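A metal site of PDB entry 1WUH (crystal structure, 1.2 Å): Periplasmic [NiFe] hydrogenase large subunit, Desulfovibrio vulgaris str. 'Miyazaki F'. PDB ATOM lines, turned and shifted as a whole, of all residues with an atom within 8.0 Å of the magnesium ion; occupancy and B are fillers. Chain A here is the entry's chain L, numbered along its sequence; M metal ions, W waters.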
ATOM      1  N   PHE A  40     -12.907 -25.546 -32.993  1.00  0.00           N
ATOM      2  CA  PHE A  40     -12.393 -24.235 -32.678  1.00  0.00           C
ATOM      3  C   PHE A  40     -13.532 -23.232 -32.648  1.00  0.00           C
ATOM      4  O   PHE A  40     -14.429 -23.301 -33.514  1.00  0.00           O
ATOM      5  CB  PHE A  40     -11.361 -23.811 -33.723  1.00  0.00           C
ATOM      6  CG  PHE A  40     -10.812 -22.415 -33.587  1.00  0.00           C
ATOM      7  CD1 PHE A  40      -9.814 -22.160 -32.668  1.00  0.00           C
ATOM      8  CD2 PHE A  40     -11.280 -21.366 -34.354  1.00  0.00           C
ATOM      9  CE1 PHE A  40      -9.250 -20.899 -32.535  1.00  0.00           C
ATOM     10  CE2 PHE A  40     -10.699 -20.112 -34.245  1.00  0.00           C
ATOM     11  CZ  PHE A  40      -9.707 -19.867 -33.345  1.00  0.00           C
ATOM     12  N   GLU A  44     -10.660 -15.758 -28.140  1.00  0.00           N
ATOM     13  CA  GLU A  44      -9.596 -14.754 -28.007  1.00  0.00           C
ATOM     14  C   GLU A  44      -9.691 -13.737 -29.157  1.00  0.00           C
ATOM     15  O   GLU A  44      -9.442 -12.554 -28.937  1.00  0.00           O
ATOM     16  CB  GLU A  44      -8.239 -15.413 -27.957  1.00  0.00           C
ATOM     17  CG  GLU A  44      -7.984 -16.287 -26.734  1.00  0.00           C
ATOM     18  CD  GLU A  44      -6.988 -17.423 -26.945  1.00  0.00           C
ATOM     19  OE1 GLU A  44      -6.806 -17.827 -28.103  1.00  0.00           O
ATOM     20  OE2 GLU A  44      -6.466 -17.893 -25.913  1.00  0.00           O
ATOM     21  N   GLU A 319       3.238 -21.077 -25.503  1.00  0.00           N
ATOM     22  CA  GLU A 319       2.303 -21.959 -26.206  1.00  0.00           C
ATOM     23  C   GLU A 319       2.765 -22.157 -27.641  1.00  0.00           C
ATOM     24  O   GLU A 319       2.860 -21.181 -28.399  1.00  0.00           O
ATOM     25  CB  GLU A 319       0.870 -21.382 -26.188  1.00  0.00           C
ATOM     26  CG  GLU A 319       0.273 -21.324 -24.809  1.00  0.00           C
ATOM     27  CD  GLU A 319      -1.156 -20.840 -24.911  1.00  0.00           C
ATOM     28  OE1 GLU A 319      -2.056 -21.728 -24.753  1.00  0.00           O
ATOM     29  OE2 GLU A 319      -1.407 -19.650 -25.167  1.00  0.00           O
ATOM     30  N   TYR A 326      -2.631 -23.472 -36.491  1.00  0.00           N
ATOM     31  CA  TYR A 326      -2.445 -22.055 -36.463  1.00  0.00           C
ATOM     32  C   TYR A 326      -1.271 -21.729 -37.388  1.00  0.00           C
ATOM     33  O   TYR A 326      -0.505 -22.590 -37.763  1.00  0.00           O
ATOM     34  CB  TYR A 326      -2.141 -21.528 -35.036  1.00  0.00           C
ATOM     35  CG  TYR A 326      -3.332 -21.839 -34.141  1.00  0.00           C
ATOM     36  CD1 TYR A 326      -3.295 -22.993 -33.333  1.00  0.00           C
ATOM     37  CD2 TYR A 326      -4.447 -21.049 -34.122  1.00  0.00           C
ATOM     38  CE1 TYR A 326      -4.373 -23.282 -32.521  1.00  0.00           C
ATOM     39  CE2 TYR A 326      -5.524 -21.357 -33.321  1.00  0.00           C
ATOM     40  CZ  TYR A 326      -5.472 -22.478 -32.515  1.00  0.00           C
ATOM     41  OH  TYR A 326      -6.576 -22.772 -31.734  1.00  0.00           O
ATOM     42  N   PRO A 334       1.885 -15.930 -23.357  1.00  0.00           N
ATOM     43  CA  PRO A 334       0.525 -15.415 -23.580  1.00  0.00           C
ATOM     44  C   PRO A 334       0.346 -13.927 -23.553  1.00  0.00           C
ATOM     45  O   PRO A 334      -0.598 -13.401 -24.140  1.00  0.00           O
ATOM     46  CB  PRO A 334      -0.277 -16.033 -22.419  1.00  0.00           C
ATOM     47  CG  PRO A 334       0.601 -16.905 -21.667  1.00  0.00           C
ATOM     48  CD  PRO A 334       1.956 -16.874 -22.239  1.00  0.00           C
ATOM     49  N   GLY A 337       0.638 -13.396 -27.055  1.00  0.00           N
ATOM     50  CA  GLY A 337       0.006 -14.515 -27.711  1.00  0.00           C
ATOM     51  C   GLY A 337      -0.578 -14.197 -29.060  1.00  0.00           C
ATOM     52  O   GLY A 337      -0.868 -13.034 -29.385  1.00  0.00           O
ATOM     53  N   GLN A 338      -0.787 -15.228 -29.884  1.00  0.00           N
ATOM     54  CA  GLN A 338      -1.373 -15.065 -31.192  1.00  0.00           C
ATOM     55  C   GLN A 338      -2.359 -16.193 -31.417  1.00  0.00           C
ATOM     56  O   GLN A 338      -2.043 -17.332 -31.050  1.00  0.00           O
ATOM     57  CB  GLN A 338      -0.310 -15.138 -32.314  1.00  0.00           C
ATOM     58  CG  GLN A 338       0.749 -14.045 -32.213  1.00  0.00           C
ATOM     59  CD  GLN A 338       1.773 -14.179 -33.330  1.00  0.00           C
ATOM     60  OE1 GLN A 338       1.913 -13.222 -34.114  1.00  0.00           O
ATOM     61  NE2 GLN A 338       2.426 -15.327 -33.375  1.00  0.00           N
ATOM     62  N   THR A 339      -3.485 -15.868 -32.031  1.00  0.00           N
ATOM     63  CA  THR A 339      -4.507 -16.889 -32.352  1.00  0.00           C
ATOM     64  C   THR A 339      -4.941 -16.684 -33.785  1.00  0.00           C
ATOM     65  O   THR A 339      -5.838 -15.919 -34.056  1.00  0.00           O
ATOM     66  CB  THR A 339      -5.645 -16.819 -31.326  1.00  0.00           C
ATOM     67  OG1 THR A 339      -5.074 -16.915 -30.029  1.00  0.00           O
ATOM     68  CG2 THR A 339      -6.641 -17.948 -31.541  1.00  0.00           C
ATOM     69  N   TRP A 354      -6.683 -28.339 -32.826  1.00  0.00           N
ATOM     70  CA  TRP A 354      -6.969 -26.929 -32.594  1.00  0.00           C
ATOM     71  C   TRP A 354      -6.421 -26.480 -31.261  1.00  0.00           C
ATOM     72  O   TRP A 354      -6.462 -25.271 -30.972  1.00  0.00           O
ATOM     73  CB  TRP A 354      -8.486 -26.643 -32.660  1.00  0.00           C
ATOM     74  CG  TRP A 354      -9.037 -26.703 -34.053  1.00  0.00           C
ATOM     75  CD1 TRP A 354      -9.889 -27.624 -34.601  1.00  0.00           C
ATOM     76  CD2 TRP A 354      -8.769 -25.752 -35.108  1.00  0.00           C
ATOM     77  NE1 TRP A 354     -10.163 -27.308 -35.910  1.00  0.00           N
ATOM     78  CE2 TRP A 354      -9.480 -26.160 -36.237  1.00  0.00           C
ATOM     79  CE3 TRP A 354      -7.994 -24.594 -35.182  1.00  0.00           C
ATOM     80  CZ2 TRP A 354      -9.436 -25.455 -37.457  1.00  0.00           C
ATOM     81  CZ3 TRP A 354      -7.945 -23.909 -36.355  1.00  0.00           C
ATOM     82  CH2 TRP A 354      -8.661 -24.330 -37.481  1.00  0.00           C
ATOM     83  N   MET A 355      -5.935 -27.336 -30.405  1.00  0.00           N
ATOM     84  CA  MET A 355      -5.281 -26.846 -29.217  1.00  0.00           C
ATOM     85  C   MET A 355      -3.852 -26.408 -29.536  1.00  0.00           C
ATOM     86  O   MET A 355      -3.161 -27.075 -30.290  1.00  0.00           O
ATOM     87  CB  MET A 355      -5.196 -27.898 -28.123  1.00  0.00           C
ATOM     88  CG  MET A 355      -6.496 -28.239 -27.437  1.00  0.00           C
ATOM     89  SD  MET A 355      -6.180 -29.131 -25.912  1.00  0.00           S
ATOM     90  CE  MET A 355      -7.786 -29.883 -25.590  1.00  0.00           C
ATOM     91  N   LYS A 356      -3.435 -25.322 -28.900  1.00  0.00           N
ATOM     92  CA  LYS A 356      -2.008 -24.991 -28.793  1.00  0.00           C
ATOM     93  C   LYS A 356      -1.344 -25.962 -27.820  1.00  0.00           C
ATOM     94  O   LYS A 356      -2.022 -26.728 -27.127  1.00  0.00           O
ATOM     95  CB  LYS A 356      -1.834 -23.566 -28.288  1.00  0.00           C
ATOM     96  CG  LYS A 356      -2.458 -22.501 -29.177  1.00  0.00           C
ATOM     97  CD  LYS A 356      -2.267 -21.098 -28.611  1.00  0.00           C
ATOM     98  CE  LYS A 356      -2.897 -20.063 -29.530  1.00  0.00           C
ATOM     99  NZ  LYS A 356      -3.014 -18.736 -28.805  1.00  0.00           N
ATOM    100  N   PRO A 358       1.044 -25.838 -24.717  1.00  0.00           N
ATOM    101  CA  PRO A 358       1.770 -25.082 -23.715  1.00  0.00           C
ATOM    102  C   PRO A 358       2.935 -25.915 -23.169  1.00  0.00           C
ATOM    103  O   PRO A 358       2.807 -27.129 -22.957  1.00  0.00           O
ATOM    104  CB  PRO A 358       0.730 -24.830 -22.628  1.00  0.00           C
ATOM    105  CG  PRO A 358      -0.599 -25.139 -23.263  1.00  0.00           C
ATOM    106  CD  PRO A 358      -0.272 -26.275 -24.227  1.00  0.00           C
ATOM    107  N   SER A 465      -5.034 -19.875 -16.560  1.00  0.00           N
ATOM    108  CA  SER A 465      -4.565 -18.491 -16.525  1.00  0.00           C
ATOM    109  C   SER A 465      -5.176 -17.733 -17.690  1.00  0.00           C
ATOM    110  O   SER A 465      -5.287 -18.233 -18.790  1.00  0.00           O
ATOM    111  CB  SER A 465      -3.055 -18.442 -16.527  1.00  0.00           C
ATOM    112  OG  SER A 465      -2.415 -19.145 -17.565  1.00  0.00           O
ATOM    113  N   TRP A 467      -4.872 -13.859 -19.498  1.00  0.00           N
ATOM    114  CA  TRP A 467      -3.835 -12.829 -19.703  1.00  0.00           C
ATOM    115  C   TRP A 467      -4.362 -11.703 -20.542  1.00  0.00           C
ATOM    116  O   TRP A 467      -4.797 -11.950 -21.637  1.00  0.00           O
ATOM    117  CB  TRP A 467      -2.663 -13.472 -20.372  1.00  0.00           C
ATOM    118  CG  TRP A 467      -2.087 -14.696 -19.719  1.00  0.00           C
ATOM    119  CD1 TRP A 467      -2.561 -15.954 -19.707  1.00  0.00           C
ATOM    120  CD2 TRP A 467      -0.879 -14.750 -18.949  1.00  0.00           C
ATOM    121  NE1 TRP A 467      -1.751 -16.796 -19.008  1.00  0.00           N
ATOM    122  CE2 TRP A 467      -0.694 -16.088 -18.532  1.00  0.00           C
ATOM    123  CE3 TRP A 467       0.095 -13.817 -18.594  1.00  0.00           C
ATOM    124  CZ2 TRP A 467       0.393 -16.480 -17.764  1.00  0.00           C
ATOM    125  CZ3 TRP A 467       1.166 -14.191 -17.842  1.00  0.00           C
ATOM    126  CH2 TRP A 467       1.284 -15.502 -17.455  1.00  0.00           C
ATOM    127  N   PHE A 478      -6.104 -10.759 -25.438  1.00  0.00           N
ATOM    128  CA  PHE A 478      -6.679 -11.546 -24.333  1.00  0.00           C
ATOM    129  C   PHE A 478      -6.363 -13.011 -24.684  1.00  0.00           C
ATOM    130  O   PHE A 478      -6.791 -13.466 -25.744  1.00  0.00           O
ATOM    131  CB  PHE A 478      -8.147 -11.305 -24.091  1.00  0.00           C
ATOM    132  CG  PHE A 478      -8.585 -11.696 -22.705  1.00  0.00           C
ATOM    133  CD1 PHE A 478      -8.683 -13.020 -22.328  1.00  0.00           C
ATOM    134  CD2 PHE A 478      -8.904 -10.728 -21.787  1.00  0.00           C
ATOM    135  CE1 PHE A 478      -9.081 -13.354 -21.042  1.00  0.00           C
ATOM    136  CE2 PHE A 478      -9.284 -11.029 -20.468  1.00  0.00           C
ATOM    137  CZ  PHE A 478      -9.351 -12.375 -20.121  1.00  0.00           C
ATOM    138  N   GLN A 479      -5.596 -13.661 -23.826  1.00  0.00           N
ATOM    139  CA  GLN A 479      -5.186 -15.039 -24.065  1.00  0.00           C
ATOM    140  C   GLN A 479      -5.589 -15.920 -22.890  1.00  0.00           C
ATOM    141  O   GLN A 479      -5.337 -15.578 -21.738  1.00  0.00           O
ATOM    142  CB  GLN A 479      -3.686 -15.112 -24.311  1.00  0.00           C
ATOM    143  CG  GLN A 479      -3.305 -14.405 -25.600  1.00  0.00           C
ATOM    144  CD  GLN A 479      -3.686 -15.129 -26.861  1.00  0.00           C
ATOM    145  OE1 GLN A 479      -3.712 -16.355 -26.951  1.00  0.00           O
ATOM    146  NE2 GLN A 479      -3.958 -14.373 -27.910  1.00  0.00           N
ATOM    147  N   LEU A 480      -6.218 -17.042 -23.246  1.00  0.00           N
ATOM    148  CA  LEU A 480      -6.525 -18.063 -22.272  1.00  0.00           C
ATOM    149  C   LEU A 480      -5.534 -19.220 -22.426  1.00  0.00           C
ATOM    150  O   LEU A 480      -5.310 -19.664 -23.518  1.00  0.00           O
ATOM    151  CB  LEU A 480      -7.941 -18.646 -22.438  1.00  0.00           C
ATOM    152  CG  LEU A 480      -9.098 -17.691 -22.240  1.00  0.00           C
ATOM    153  CD1 LEU A 480      -9.250 -16.668 -23.316  1.00  0.00           C
ATOM    154  CD2 LEU A 480     -10.408 -18.540 -22.201  1.00  0.00           C
ATOM    155  N   VAL A 481      -4.970 -19.686 -21.314  1.00  0.00           N
ATOM    156  CA  VAL A 481      -4.120 -20.870 -21.299  1.00  0.00           C
ATOM    157  C   VAL A 481      -4.789 -21.795 -20.287  1.00  0.00           C
ATOM    158  O   VAL A 481      -4.858 -21.464 -19.104  1.00  0.00           O
ATOM    159  CB  VAL A 481      -2.669 -20.584 -20.922  1.00  0.00           C
ATOM    160  CG1 VAL A 481      -1.832 -21.862 -21.090  1.00  0.00           C
ATOM    161  CG2 VAL A 481      -2.114 -19.453 -21.781  1.00  0.00           C
ATOM    162  N   VAL A 482      -5.363 -22.919 -20.762  1.00  0.00           N
ATOM    163  CA  VAL A 482      -6.355 -23.622 -19.959  1.00  0.00           C
ATOM    164  C   VAL A 482      -5.812 -24.972 -19.545  1.00  0.00           C
ATOM    165  O   VAL A 482      -4.942 -25.499 -20.236  1.00  0.00           O
ATOM    166  CB  VAL A 482      -7.652 -23.681 -20.785  1.00  0.00           C
ATOM    167  CG1 VAL A 482      -8.861 -24.255 -20.110  1.00  0.00           C
ATOM    168  CG2 VAL A 482      -8.052 -22.242 -21.148  1.00  0.00           C
ATOM    169  N   THR A 485      -5.542 -27.579 -22.134  1.00  0.00           N
ATOM    170  CA  THR A 485      -4.534 -27.241 -23.127  1.00  0.00           C
ATOM    171  C   THR A 485      -3.181 -27.822 -22.756  1.00  0.00           C
ATOM    172  O   THR A 485      -2.526 -28.432 -23.589  1.00  0.00           O
ATOM    173  CB  THR A 485      -4.407 -25.698 -23.306  1.00  0.00           C
ATOM    174  OG1 THR A 485      -5.667 -25.049 -23.194  1.00  0.00           O
ATOM    175  CG2 THR A 485      -3.799 -25.354 -24.632  1.00  0.00           C
ATOM    176  N   CYS A 531     -12.758 -25.973 -23.209  1.00  0.00           N
ATOM    177  CA  CYS A 531     -11.686 -25.338 -22.412  1.00  0.00           C
ATOM    178  C   CYS A 531     -10.385 -25.320 -23.163  1.00  0.00           C
ATOM    179  O   CYS A 531      -9.730 -24.278 -23.265  1.00  0.00           O
ATOM    180  CB  CYS A 531     -11.471 -26.128 -21.067  1.00  0.00           C
ATOM    181  SG  CYS A 531     -12.486 -25.446 -19.781  1.00  0.00           S
ATOM    182  N   GLY A 532      -9.951 -26.478 -23.658  1.00  0.00           N
ATOM    183  CA  GLY A 532      -8.581 -26.523 -24.166  1.00  0.00           C
ATOM    184  C   GLY A 532      -8.343 -25.656 -25.389  1.00  0.00           C
ATOM    185  O   GLY A 532      -7.243 -25.145 -25.561  1.00  0.00           O
ATOM    186  N   VAL A 533      -9.375 -25.541 -26.233  1.00  0.00           N
ATOM    187  CA  VAL A 533      -9.243 -24.804 -27.490  1.00  0.00           C
ATOM    188  C   VAL A 533      -9.803 -23.410 -27.418  1.00  0.00           C
ATOM    189  O   VAL A 533      -9.179 -22.453 -27.944  1.00  0.00           O
ATOM    190  CB  VAL A 533      -9.983 -25.512 -28.653  1.00  0.00           C
ATOM    191  CG1 VAL A 533      -9.866 -24.744 -29.988  1.00  0.00           C
ATOM    192  CG2 VAL A 533      -9.486 -26.930 -28.818  1.00  0.00           C
ATOM    193  N   HIS A 534     -10.961 -23.166 -26.785  1.00  0.00           N
ATOM    194  CA  HIS A 534     -11.651 -21.858 -26.738  1.00  0.00           C
ATOM    195  C   HIS A 534     -11.656 -21.184 -28.111  1.00  0.00           C
ATOM    196  O   HIS A 534     -12.002 -21.976 -29.115  1.00  0.00           O
ATOM    197  CB  HIS A 534     -11.146 -20.960 -25.601  1.00  0.00           C
ATOM    198  CG  HIS A 534      -9.666 -20.943 -25.394  1.00  0.00           C
ATOM    199  ND1 HIS A 534      -9.009 -21.968 -24.731  1.00  0.00           N
ATOM    200  CD2 HIS A 534      -8.680 -20.154 -25.825  1.00  0.00           C
ATOM    201  CE1 HIS A 534      -7.708 -21.750 -24.732  1.00  0.00           C
ATOM    202  NE2 HIS A 534      -7.465 -20.636 -25.399  1.00  0.00           N
ATOM    203  OXT HIS A 534     -11.446 -19.998 -28.244  1.00  0.00           O
HETATM  204 MG    MG M   1      -5.499 -19.784 -25.659  1.00  0.00          MG
HETATM  205  O   HOH W   1      -3.723 -18.805 -25.846  1.00  0.00           O
HETATM  206  O   HOH W   2      -4.550 -21.628 -25.464  1.00  0.00           O
HETATM  207  O   HOH W   3      -5.540 -20.053 -27.708  1.00  0.00           O
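Three residues have an atom within 4 Å of the magnesium ion: Glu 44, Leu 480 and His 534. The nearest printed residue that does not touch the magnesium ion is Glu 319 (4.1 Å).
The magnesium ion is bound by water W1, at 2.0 Å. The magnesium ion is bound by water W3, 2.1 Å away. Water W2 binds the magnesium ion (2.1 Å). The magnesium ion is bound by OE2 of Glu 44 (2.1 Å). The magnesium ion is bound by the backbone carbonyl oxygen (O) of Leu 480 (2.2 Å). The magnesium ion is bound by NE2 of His 534, at 2.2 Å. The magnesium ion has six donor atoms within binding distance.
OE2 of Glu 44 sits close to OE1 of Gln 479 (3.3 Å). OE1 of Glu 44 is in salt-bridge range of NZ of Lys 356, 3.96 Å away. The side-chain hydroxyl (OG1) of Thr 339 is in hydrogen-bond range of the side-chain carboxylate (OE1) of Glu 44 (2.7 Å). A ring nitrogen (ND1) of His 534 lies within hydrogen-bond range of the backbone carbonyl oxygen (O) of Cys 531 (2.8 Å).
Water W3 lies within hydrogen-bond range of OE1 of Glu 44 (2.6 Å) and NZ of Lys 356 (3.1 Å). Water W1 lies within hydrogen-bond range of OE2 of Glu 319, OE1 of Gln 479 and NZ of Lys 356.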
